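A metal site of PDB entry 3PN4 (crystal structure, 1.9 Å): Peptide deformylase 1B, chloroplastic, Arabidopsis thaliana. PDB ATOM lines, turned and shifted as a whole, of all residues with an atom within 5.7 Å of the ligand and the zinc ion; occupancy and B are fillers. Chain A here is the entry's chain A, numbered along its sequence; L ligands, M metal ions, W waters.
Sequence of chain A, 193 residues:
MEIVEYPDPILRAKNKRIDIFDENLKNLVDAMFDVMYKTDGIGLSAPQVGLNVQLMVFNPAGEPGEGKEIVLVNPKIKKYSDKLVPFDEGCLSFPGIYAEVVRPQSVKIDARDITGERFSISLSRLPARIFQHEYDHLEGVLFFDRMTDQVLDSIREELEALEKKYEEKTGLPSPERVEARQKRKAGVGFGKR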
ATOM      1  N   THR A  39     -14.761 -18.200 -16.435  1.00  0.00           N
ATOM      2  CA  THR A  39     -15.708 -19.246 -16.880  1.00  0.00           C
ATOM      3  C   THR A  39     -16.577 -19.791 -15.726  1.00  0.00           C
ATOM      4  O   THR A  39     -17.317 -20.758 -15.907  1.00  0.00           O
ATOM      5  CB  THR A  39     -14.986 -20.410 -17.614  1.00  0.00           C
ATOM      6  OG1 THR A  39     -14.079 -21.075 -16.712  1.00  0.00           O
ATOM      7  CG2 THR A  39     -14.209 -19.865 -18.842  1.00  0.00           C
ATOM      8  N   ASP A  40     -16.436 -19.191 -14.556  1.00  0.00           N
ATOM      9  CA  ASP A  40     -17.172 -19.598 -13.377  1.00  0.00           C
ATOM     10  C   ASP A  40     -16.875 -21.007 -12.876  1.00  0.00           C
ATOM     11  O   ASP A  40     -17.794 -21.669 -12.361  1.00  0.00           O
ATOM     12  CB  ASP A  40     -18.652 -19.459 -13.585  1.00  0.00           C
ATOM     13  CG  ASP A  40     -19.163 -18.234 -12.982  1.00  0.00           C
ATOM     14  OD1 ASP A  40     -18.938 -17.148 -13.578  1.00  0.00           O
ATOM     15  OD2 ASP A  40     -19.751 -18.342 -11.878  1.00  0.00           O
ATOM     16  N   GLY A  41     -15.629 -21.420 -12.983  1.00  0.00           N
ATOM     17  CA  GLY A  41     -15.176 -22.670 -12.405  1.00  0.00           C
ATOM     18  C   GLY A  41     -14.666 -22.539 -10.989  1.00  0.00           C
ATOM     19  O   GLY A  41     -14.581 -21.443 -10.435  1.00  0.00           O
ATOM     20  N   ILE A  42     -14.335 -23.673 -10.378  1.00  0.00           N
ATOM     21  CA  ILE A  42     -13.750 -23.658  -9.033  1.00  0.00           C
ATOM     22  C   ILE A  42     -12.395 -24.395  -9.051  1.00  0.00           C
ATOM     23  O   ILE A  42     -11.746 -24.565  -8.017  1.00  0.00           O
ATOM     24  CB  ILE A  42     -14.761 -24.223  -7.959  1.00  0.00           C
ATOM     25  CG1 ILE A  42     -15.121 -25.687  -8.288  1.00  0.00           C
ATOM     26  CG2 ILE A  42     -16.019 -23.301  -7.889  1.00  0.00           C
ATOM     27  CD1 ILE A  42     -16.097 -26.382  -7.335  1.00  0.00           C
ATOM     28  N   GLY A  43     -11.993 -24.874 -10.238  1.00  0.00           N
ATOM     29  CA  GLY A  43     -10.678 -25.474 -10.389  1.00  0.00           C
ATOM     30  C   GLY A  43     -10.342 -25.596 -11.864  1.00  0.00           C
ATOM     31  O   GLY A  43     -11.210 -25.385 -12.711  1.00  0.00           O
ATOM     32  N   LEU A  44      -9.082 -25.918 -12.169  1.00  0.00           N
ATOM     33  CA  LEU A  44      -8.692 -26.142 -13.554  1.00  0.00           C
ATOM     34  C   LEU A  44      -7.390 -26.934 -13.586  1.00  0.00           C
ATOM     35  O   LEU A  44      -6.541 -26.768 -12.718  1.00  0.00           O
ATOM     36  CB  LEU A  44      -8.490 -24.790 -14.306  1.00  0.00           C
ATOM     37  CG  LEU A  44      -8.456 -24.815 -15.830  1.00  0.00           C
ATOM     38  CD1 LEU A  44      -9.816 -25.296 -16.429  1.00  0.00           C
ATOM     39  CD2 LEU A  44      -8.038 -23.411 -16.408  1.00  0.00           C
ATOM     40  N   SER A  45      -7.239 -27.770 -14.625  1.00  0.00           N
ATOM     41  CA  SER A  45      -6.031 -28.553 -14.818  1.00  0.00           C
ATOM     42  C   SER A  45      -5.361 -28.151 -16.133  1.00  0.00           C
ATOM     43  O   SER A  45      -6.028 -27.710 -17.079  1.00  0.00           O
ATOM     44  CB  SER A  45      -6.356 -30.054 -14.800  1.00  0.00           C
ATOM     45  OG  SER A  45      -7.100 -30.394 -15.985  1.00  0.00           O
ATOM     46  N   GLN A  48      -6.522 -28.958 -19.716  1.00  0.00           N
ATOM     47  CA  GLN A  48      -7.747 -28.274 -20.132  1.00  0.00           C
ATOM     48  C   GLN A  48      -7.497 -26.953 -20.827  1.00  0.00           C
ATOM     49  O   GLN A  48      -8.422 -26.409 -21.424  1.00  0.00           O
ATOM     50  CB  GLN A  48      -8.684 -28.076 -18.939  1.00  0.00           C
ATOM     51  CG  GLN A  48      -9.314 -29.402 -18.454  1.00  0.00           C
ATOM     52  CD  GLN A  48     -10.196 -29.157 -17.254  1.00  0.00           C
ATOM     53  OE1 GLN A  48      -9.706 -28.991 -16.131  1.00  0.00           O
ATOM     54  NE2 GLN A  48     -11.524 -29.086 -17.485  1.00  0.00           N
ATOM     55  N   PHE A  87     -22.048 -36.186  -5.357  1.00  0.00           N
ATOM     56  CA  PHE A  87     -22.070 -34.737  -5.583  1.00  0.00           C
ATOM     57  C   PHE A  87     -22.269 -34.500  -7.069  1.00  0.00           C
ATOM     58  O   PHE A  87     -21.702 -35.217  -7.892  1.00  0.00           O
ATOM     59  CB  PHE A  87     -20.764 -34.078  -5.107  1.00  0.00           C
ATOM     60  CG  PHE A  87     -20.840 -32.562  -4.954  1.00  0.00           C
ATOM     61  CD1 PHE A  87     -21.490 -31.987  -3.852  1.00  0.00           C
ATOM     62  CD2 PHE A  87     -20.238 -31.729  -5.882  1.00  0.00           C
ATOM     63  CE1 PHE A  87     -21.552 -30.581  -3.697  1.00  0.00           C
ATOM     64  CE2 PHE A  87     -20.281 -30.319  -5.737  1.00  0.00           C
ATOM     65  CZ  PHE A  87     -20.945 -29.747  -4.655  1.00  0.00           C
ATOM     66  N   ASP A  88     -23.093 -33.493  -7.416  1.00  0.00           N
ATOM     67  CA  ASP A  88     -23.312 -33.159  -8.814  1.00  0.00           C
ATOM     68  C   ASP A  88     -22.140 -32.364  -9.332  1.00  0.00           C
ATOM     69  O   ASP A  88     -21.872 -31.281  -8.828  1.00  0.00           O
ATOM     70  CB  ASP A  88     -24.613 -32.374  -9.005  1.00  0.00           C
ATOM     71  CG  ASP A  88     -25.851 -33.261  -8.868  1.00  0.00           C
ATOM     72  OD1 ASP A  88     -25.714 -34.482  -8.644  1.00  0.00           O
ATOM     73  OD2 ASP A  88     -26.972 -32.734  -8.990  1.00  0.00           O
ATOM     74  N   GLU A  89     -21.457 -32.917 -10.334  1.00  0.00           N
ATOM     75  CA  GLU A  89     -20.304 -32.254 -10.951  1.00  0.00           C
ATOM     76  C   GLU A  89     -20.645 -31.764 -12.359  1.00  0.00           C
ATOM     77  O   GLU A  89     -21.456 -32.360 -13.061  1.00  0.00           O
ATOM     78  CB  GLU A  89     -19.134 -33.223 -11.059  1.00  0.00           C
ATOM     79  CG  GLU A  89     -18.604 -33.678  -9.689  1.00  0.00           C
ATOM     80  CD  GLU A  89     -17.313 -34.474  -9.783  1.00  0.00           C
ATOM     81  OE1 GLU A  89     -16.959 -35.122  -8.770  1.00  0.00           O
ATOM     82  OE2 GLU A  89     -16.626 -34.456 -10.835  1.00  0.00           O
ATOM     83  N   GLY A  90     -20.010 -30.661 -12.743  1.00  0.00           N
ATOM     84  CA  GLY A  90     -19.843 -30.282 -14.155  1.00  0.00           C
ATOM     85  C   GLY A  90     -18.336 -30.228 -14.415  1.00  0.00           C
ATOM     86  O   GLY A  90     -17.501 -30.293 -13.494  1.00  0.00           O
ATOM     87  N   CYS A  91     -17.969 -30.070 -15.680  1.00  0.00           N
ATOM     88  CA  CYS A  91     -16.575 -29.971 -16.027  1.00  0.00           C
ATOM     89  C   CYS A  91     -16.507 -28.964 -17.138  1.00  0.00           C
ATOM     90  O   CYS A  91     -17.316 -29.011 -18.066  1.00  0.00           O
ATOM     91  CB  CYS A  91     -16.021 -31.346 -16.466  1.00  0.00           C
ATOM     92  SG  CYS A  91     -14.360 -31.361 -17.161  1.00  0.00           S
ATOM     93  N   LEU A  92     -15.538 -28.042 -17.059  1.00  0.00           N
ATOM     94  CA  LEU A  92     -15.397 -27.022 -18.088  1.00  0.00           C
ATOM     95  C   LEU A  92     -15.078 -27.624 -19.461  1.00  0.00           C
ATOM     96  O   LEU A  92     -15.298 -26.961 -20.487  1.00  0.00           O
ATOM     97  CB  LEU A  92     -14.306 -26.016 -17.670  1.00  0.00           C
ATOM     98  CG  LEU A  92     -14.692 -25.104 -16.519  1.00  0.00           C
ATOM     99  CD1 LEU A  92     -13.462 -24.232 -16.061  1.00  0.00           C
ATOM    100  CD2 LEU A  92     -15.883 -24.225 -16.957  1.00  0.00           C
ATOM    101  N   SER A  93     -14.595 -28.863 -19.495  1.00  0.00           N
ATOM    102  CA  SER A  93     -14.337 -29.545 -20.782  1.00  0.00           C
ATOM    103  C   SER A  93     -15.612 -30.182 -21.373  1.00  0.00           C
ATOM    104  O   SER A  93     -15.591 -30.774 -22.457  1.00  0.00           O
ATOM    105  CB  SER A  93     -13.232 -30.620 -20.641  1.00  0.00           C
ATOM    106  OG  SER A  93     -11.987 -30.021 -20.284  1.00  0.00           O
ATOM    107  N   ILE A  97     -22.960 -29.854 -19.110  1.00  0.00           N
ATOM    108  CA  ILE A  97     -23.274 -31.220 -18.660  1.00  0.00           C
ATOM    109  C   ILE A  97     -23.027 -31.328 -17.165  1.00  0.00           C
ATOM    110  O   ILE A  97     -21.938 -31.021 -16.697  1.00  0.00           O
ATOM    111  CB  ILE A  97     -22.439 -32.307 -19.421  1.00  0.00           C
ATOM    112  CG1 ILE A  97     -22.719 -32.233 -20.942  1.00  0.00           C
ATOM    113  CG2 ILE A  97     -22.747 -33.724 -18.883  1.00  0.00           C
ATOM    114  CD1 ILE A  97     -21.865 -33.173 -21.772  1.00  0.00           C
ATOM    115  N   TYR A  98     -24.051 -31.735 -16.418  1.00  0.00           N
ATOM    116  CA  TYR A  98     -23.918 -31.926 -14.967  1.00  0.00           C
ATOM    117  C   TYR A  98     -24.485 -33.271 -14.632  1.00  0.00           C
ATOM    118  O   TYR A  98     -25.553 -33.633 -15.121  1.00  0.00           O
ATOM    119  CB  TYR A  98     -24.719 -30.866 -14.191  1.00  0.00           C
ATOM    120  CG  TYR A  98     -24.254 -29.469 -14.493  1.00  0.00           C
ATOM    121  CD1 TYR A  98     -24.840 -28.744 -15.532  1.00  0.00           C
ATOM    122  CD2 TYR A  98     -23.207 -28.889 -13.783  1.00  0.00           C
ATOM    123  CE1 TYR A  98     -24.411 -27.442 -15.842  1.00  0.00           C
ATOM    124  CE2 TYR A  98     -22.770 -27.599 -14.092  1.00  0.00           C
ATOM    125  CZ  TYR A  98     -23.376 -26.896 -15.118  1.00  0.00           C
ATOM    126  OH  TYR A  98     -22.946 -25.628 -15.423  1.00  0.00           O
ATOM    127  N   LEU A 126     -15.488 -30.004   0.138  1.00  0.00           N
ATOM    128  CA  LEU A 126     -15.396 -29.536  -1.235  1.00  0.00           C
ATOM    129  C   LEU A 126     -13.951 -29.563  -1.778  1.00  0.00           C
ATOM    130  O   LEU A 126     -13.749 -29.996  -2.896  1.00  0.00           O
ATOM    131  CB  LEU A 126     -16.053 -28.158  -1.419  1.00  0.00           C
ATOM    132  CG  LEU A 126     -16.205 -27.624  -2.844  1.00  0.00           C
ATOM    133  CD1 LEU A 126     -16.921 -28.642  -3.741  1.00  0.00           C
ATOM    134  CD2 LEU A 126     -16.976 -26.299  -2.780  1.00  0.00           C
ATOM    135  N   ARG A 129     -13.117 -32.868  -3.015  1.00  0.00           N
ATOM    136  CA  ARG A 129     -13.937 -33.149  -4.193  1.00  0.00           C
ATOM    137  C   ARG A 129     -13.326 -32.505  -5.424  1.00  0.00           C
ATOM    138  O   ARG A 129     -13.124 -33.189  -6.429  1.00  0.00           O
ATOM    139  CB  ARG A 129     -15.375 -32.640  -3.990  1.00  0.00           C
ATOM    140  CG  ARG A 129     -16.237 -32.646  -5.279  1.00  0.00           C
ATOM    141  CD  ARG A 129     -16.384 -34.002  -5.957  1.00  0.00           C
ATOM    142  NE  ARG A 129     -16.859 -35.013  -5.009  1.00  0.00           N
ATOM    143  CZ  ARG A 129     -17.750 -35.954  -5.276  1.00  0.00           C
ATOM    144  NH1 ARG A 129     -18.299 -36.047  -6.490  1.00  0.00           N
ATOM    145  NH2 ARG A 129     -18.134 -36.787  -4.318  1.00  0.00           N
ATOM    146  N   ILE A 130     -13.024 -31.204  -5.335  1.00  0.00           N
ATOM    147  CA  ILE A 130     -12.355 -30.510  -6.436  1.00  0.00           C
ATOM    148  C   ILE A 130     -11.029 -31.184  -6.750  1.00  0.00           C
ATOM    149  O   ILE A 130     -10.705 -31.405  -7.940  1.00  0.00           O
ATOM    150  CB  ILE A 130     -12.082 -29.022  -6.143  1.00  0.00           C
ATOM    151  CG1 ILE A 130     -13.382 -28.278  -5.830  1.00  0.00           C
ATOM    152  CG2 ILE A 130     -11.369 -28.374  -7.344  1.00  0.00           C
ATOM    153  CD1 ILE A 130     -13.142 -26.913  -5.101  1.00  0.00           C
ATOM    154  N   HIS A 133     -11.403 -34.488  -8.793  1.00  0.00           N
ATOM    155  CA  HIS A 133     -11.794 -34.136 -10.186  1.00  0.00           C
ATOM    156  C   HIS A 133     -10.570 -33.680 -10.996  1.00  0.00           C
ATOM    157  O   HIS A 133     -10.340 -34.163 -12.138  1.00  0.00           O
ATOM    158  CB  HIS A 133     -12.871 -33.048 -10.174  1.00  0.00           C
ATOM    159  CG  HIS A 133     -13.364 -32.644 -11.534  1.00  0.00           C
ATOM    160  ND1 HIS A 133     -14.601 -33.013 -12.023  1.00  0.00           N
ATOM    161  CD2 HIS A 133     -12.777 -31.894 -12.505  1.00  0.00           C
ATOM    162  CE1 HIS A 133     -14.753 -32.515 -13.240  1.00  0.00           C
ATOM    163  NE2 HIS A 133     -13.665 -31.833 -13.556  1.00  0.00           N
ATOM    164  N   GLU A 134      -9.776 -32.768 -10.437  1.00  0.00           N
ATOM    165  CA  GLU A 134      -8.597 -32.216 -11.156  1.00  0.00           C
ATOM    166  C   GLU A 134      -7.493 -33.248 -11.259  1.00  0.00           C
ATOM    167  O   GLU A 134      -6.750 -33.291 -12.251  1.00  0.00           O
ATOM    168  CB  GLU A 134      -7.998 -30.981 -10.437  1.00  0.00           C
ATOM    169  CG  GLU A 134      -8.905 -29.779 -10.263  1.00  0.00           C
ATOM    170  CD  GLU A 134      -9.559 -29.292 -11.544  1.00  0.00           C
ATOM    171  OE1 GLU A 134      -8.966 -29.388 -12.644  1.00  0.00           O
ATOM    172  OE2 GLU A 134     -10.719 -28.800 -11.417  1.00  0.00           O
ATOM    173  N   HIS A 137      -8.076 -35.501 -14.104  1.00  0.00           N
ATOM    174  CA  HIS A 137      -7.627 -34.870 -15.369  1.00  0.00           C
ATOM    175  C   HIS A 137      -6.127 -35.094 -15.583  1.00  0.00           C
ATOM    176  O   HIS A 137      -5.650 -35.315 -16.699  1.00  0.00           O
ATOM    177  CB  HIS A 137      -7.853 -33.364 -15.354  1.00  0.00           C
ATOM    178  CG  HIS A 137      -9.235 -32.938 -15.773  1.00  0.00           C
ATOM    179  ND1 HIS A 137      -9.723 -33.139 -17.042  1.00  0.00           N
ATOM    180  CD2 HIS A 137     -10.218 -32.324 -15.075  1.00  0.00           C
ATOM    181  CE1 HIS A 137     -10.940 -32.625 -17.135  1.00  0.00           C
ATOM    182  NE2 HIS A 137     -11.264 -32.118 -15.956  1.00  0.00           N
HETATM  183  C1  LIG L   1     -13.775 -27.261 -13.462  1.00  0.00           C
HETATM  184  C2  LIG L   1     -13.052 -28.338 -14.196  1.00  0.00           C
HETATM  185  O1  LIG L   1     -13.509 -28.872 -15.206  1.00  0.00           O
HETATM  186  N1  LIG L   1     -11.900 -28.727 -13.653  1.00  0.00           N
HETATM  187  O2  LIG L   1     -11.261 -29.752 -14.283  1.00  0.00           O
HETATM  188  C3  LIG L   1     -14.857 -27.915 -12.574  1.00  0.00           C
HETATM  189  C4  LIG L   1     -15.912 -26.871 -12.183  1.00  0.00           C
HETATM  190  O3  LIG L   1     -15.624 -25.713 -11.794  1.00  0.00           O
HETATM  191  C5  LIG L   1     -14.238 -28.502 -11.266  1.00  0.00           C
HETATM  192  C6  LIG L   1     -15.313 -29.390 -10.557  1.00  0.00           C
HETATM  193  C7  LIG L   1     -14.814 -29.910  -9.193  1.00  0.00           C
HETATM  194  C8  LIG L   1     -15.716 -31.061  -8.673  1.00  0.00           C
HETATM  195  C9  LIG L   1     -16.963 -30.470  -8.003  1.00  0.00           C
HETATM  196  N2  LIG L   1     -17.162 -27.310 -12.311  1.00  0.00           N
HETATM  197  C10 LIG L   1     -18.298 -26.486 -11.909  1.00  0.00           C
HETATM  198  C11 LIG L   1     -19.159 -25.929 -13.074  1.00  0.00           C
HETATM  199  C12 LIG L   1     -18.326 -25.038 -14.012  1.00  0.00           C
HETATM  200  C13 LIG L   1     -19.814 -27.029 -13.901  1.00  0.00           C
HETATM  201  C14 LIG L   1     -19.064 -27.376 -10.893  1.00  0.00           C
HETATM  202  O4  LIG L   1     -19.145 -28.597 -11.067  1.00  0.00           O
HETATM  203  N3  LIG L   1     -19.596 -26.821  -9.774  1.00  0.00           N
HETATM  204  C15 LIG L   1     -20.319 -27.572  -8.700  1.00  0.00           C
HETATM  205  C16 LIG L   1     -19.507 -25.368  -9.473  1.00  0.00           C
HETATM  206  C17 LIG L   1     -20.143 -25.178  -8.079  1.00  0.00           C
HETATM  207  C18 LIG L   1     -20.315 -26.599  -7.501  1.00  0.00           C
HETATM  208  C19 LIG L   1     -21.767 -27.910  -9.108  1.00  0.00           C
HETATM  209  O5  LIG L   1     -22.390 -28.744  -8.113  1.00  0.00           O
HETATM  210 ZN    ZN M   1     -12.985 -30.964 -15.345  1.00  0.00          ZN
HETATM  211  O   HOH W   1     -23.877 -28.153  -5.822  1.00  0.00           O
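A nitrogen (N1) of the ligand is in hydrogen-bond range of the side-chain carboxylate (OE2) of Glu 134. The side-chain amide oxygen (OE1) of Gln 48 is in hydrogen-bond range of a nitrogen (N1) of the ligand (3.3 Å). The backbone carbonyl oxygen (O) of Asp 88 sits at hydrogen-bond distance from an oxygen (O5) of the ligand (2.7 Å). N of Gly 90 sits at hydrogen-bond distance from O4 of the ligand (2.8 Å). The backbone carbonyl oxygen (O) of Gly 90 lies within hydrogen-bond range of a nitrogen (N2) of the ligand (3.2 Å). The backbone NH (N) of Ile 42 lies within hydrogen-bond range of an oxygen (O3) of the ligand (2.8 Å). The backbone NH (N) of Leu 92 lies close to an oxygen (O1) of the ligand, at 2.9 Å.
A ring nitrogen (ND1) of His 133 is in hydrogen-bond range of the side-chain carboxylate (OE2) of Glu 89 (2.8 Å). The side-chain sulfur of Cys 91 lies close to the side-chain amide nitrogen of Gln 48, at 3.7 Å. The side-chain sulfur (SG) of Cys 91 sits close to the backbone NH (N) of Ser 93, 3.4 Å away. N of Leu 44 lies within hydrogen-bond range of OE2 of Glu 134 (3.4 Å). N of Ser 45 sits at hydrogen-bond distance from OE1 of Glu 134 (3.1 Å). OG of Ser 93 sits at hydrogen-bond distance from NE2 of Gln 48. The side-chain amide oxygen (OE1) of Gln 48 lies within hydrogen-bond range of the side-chain hydroxyl (OG) of Ser 45. The side-chain carboxylate (OE1) of Glu 89 lies within salt-bridge range of the guanidinium group (NH1) of Arg 129, 2.8 Å away.
Residues that only touch the ligand: Asp 40 (3.8 Å), Gly 41 (3.1 Å), Gly 43 (3.3 Å), Phe 87 (3.5 Å), Glu 89 (3.7 Å), Tyr 98 (3.0 Å), Arg 129 (3.6 Å) and Ile 130 (3.7 Å).
Gln 48 touches the zinc ion (NE2 to ZN, 3.2 Å). Of the 23 residues printed, 4 come within 4 Å of the zinc ion.
A ring nitrogen (NE2) of His 133 is bound to the zinc ion. The zinc ion is bound by NE2 of His 137. The zinc ion is bound by an oxygen (O1) of the ligand. SG of Cys 91 binds the zinc ion (2.3 Å). An oxygen (O2) of the ligand binds the zinc ion (2.4 Å). The zinc ion has five donor atoms within binding distance.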
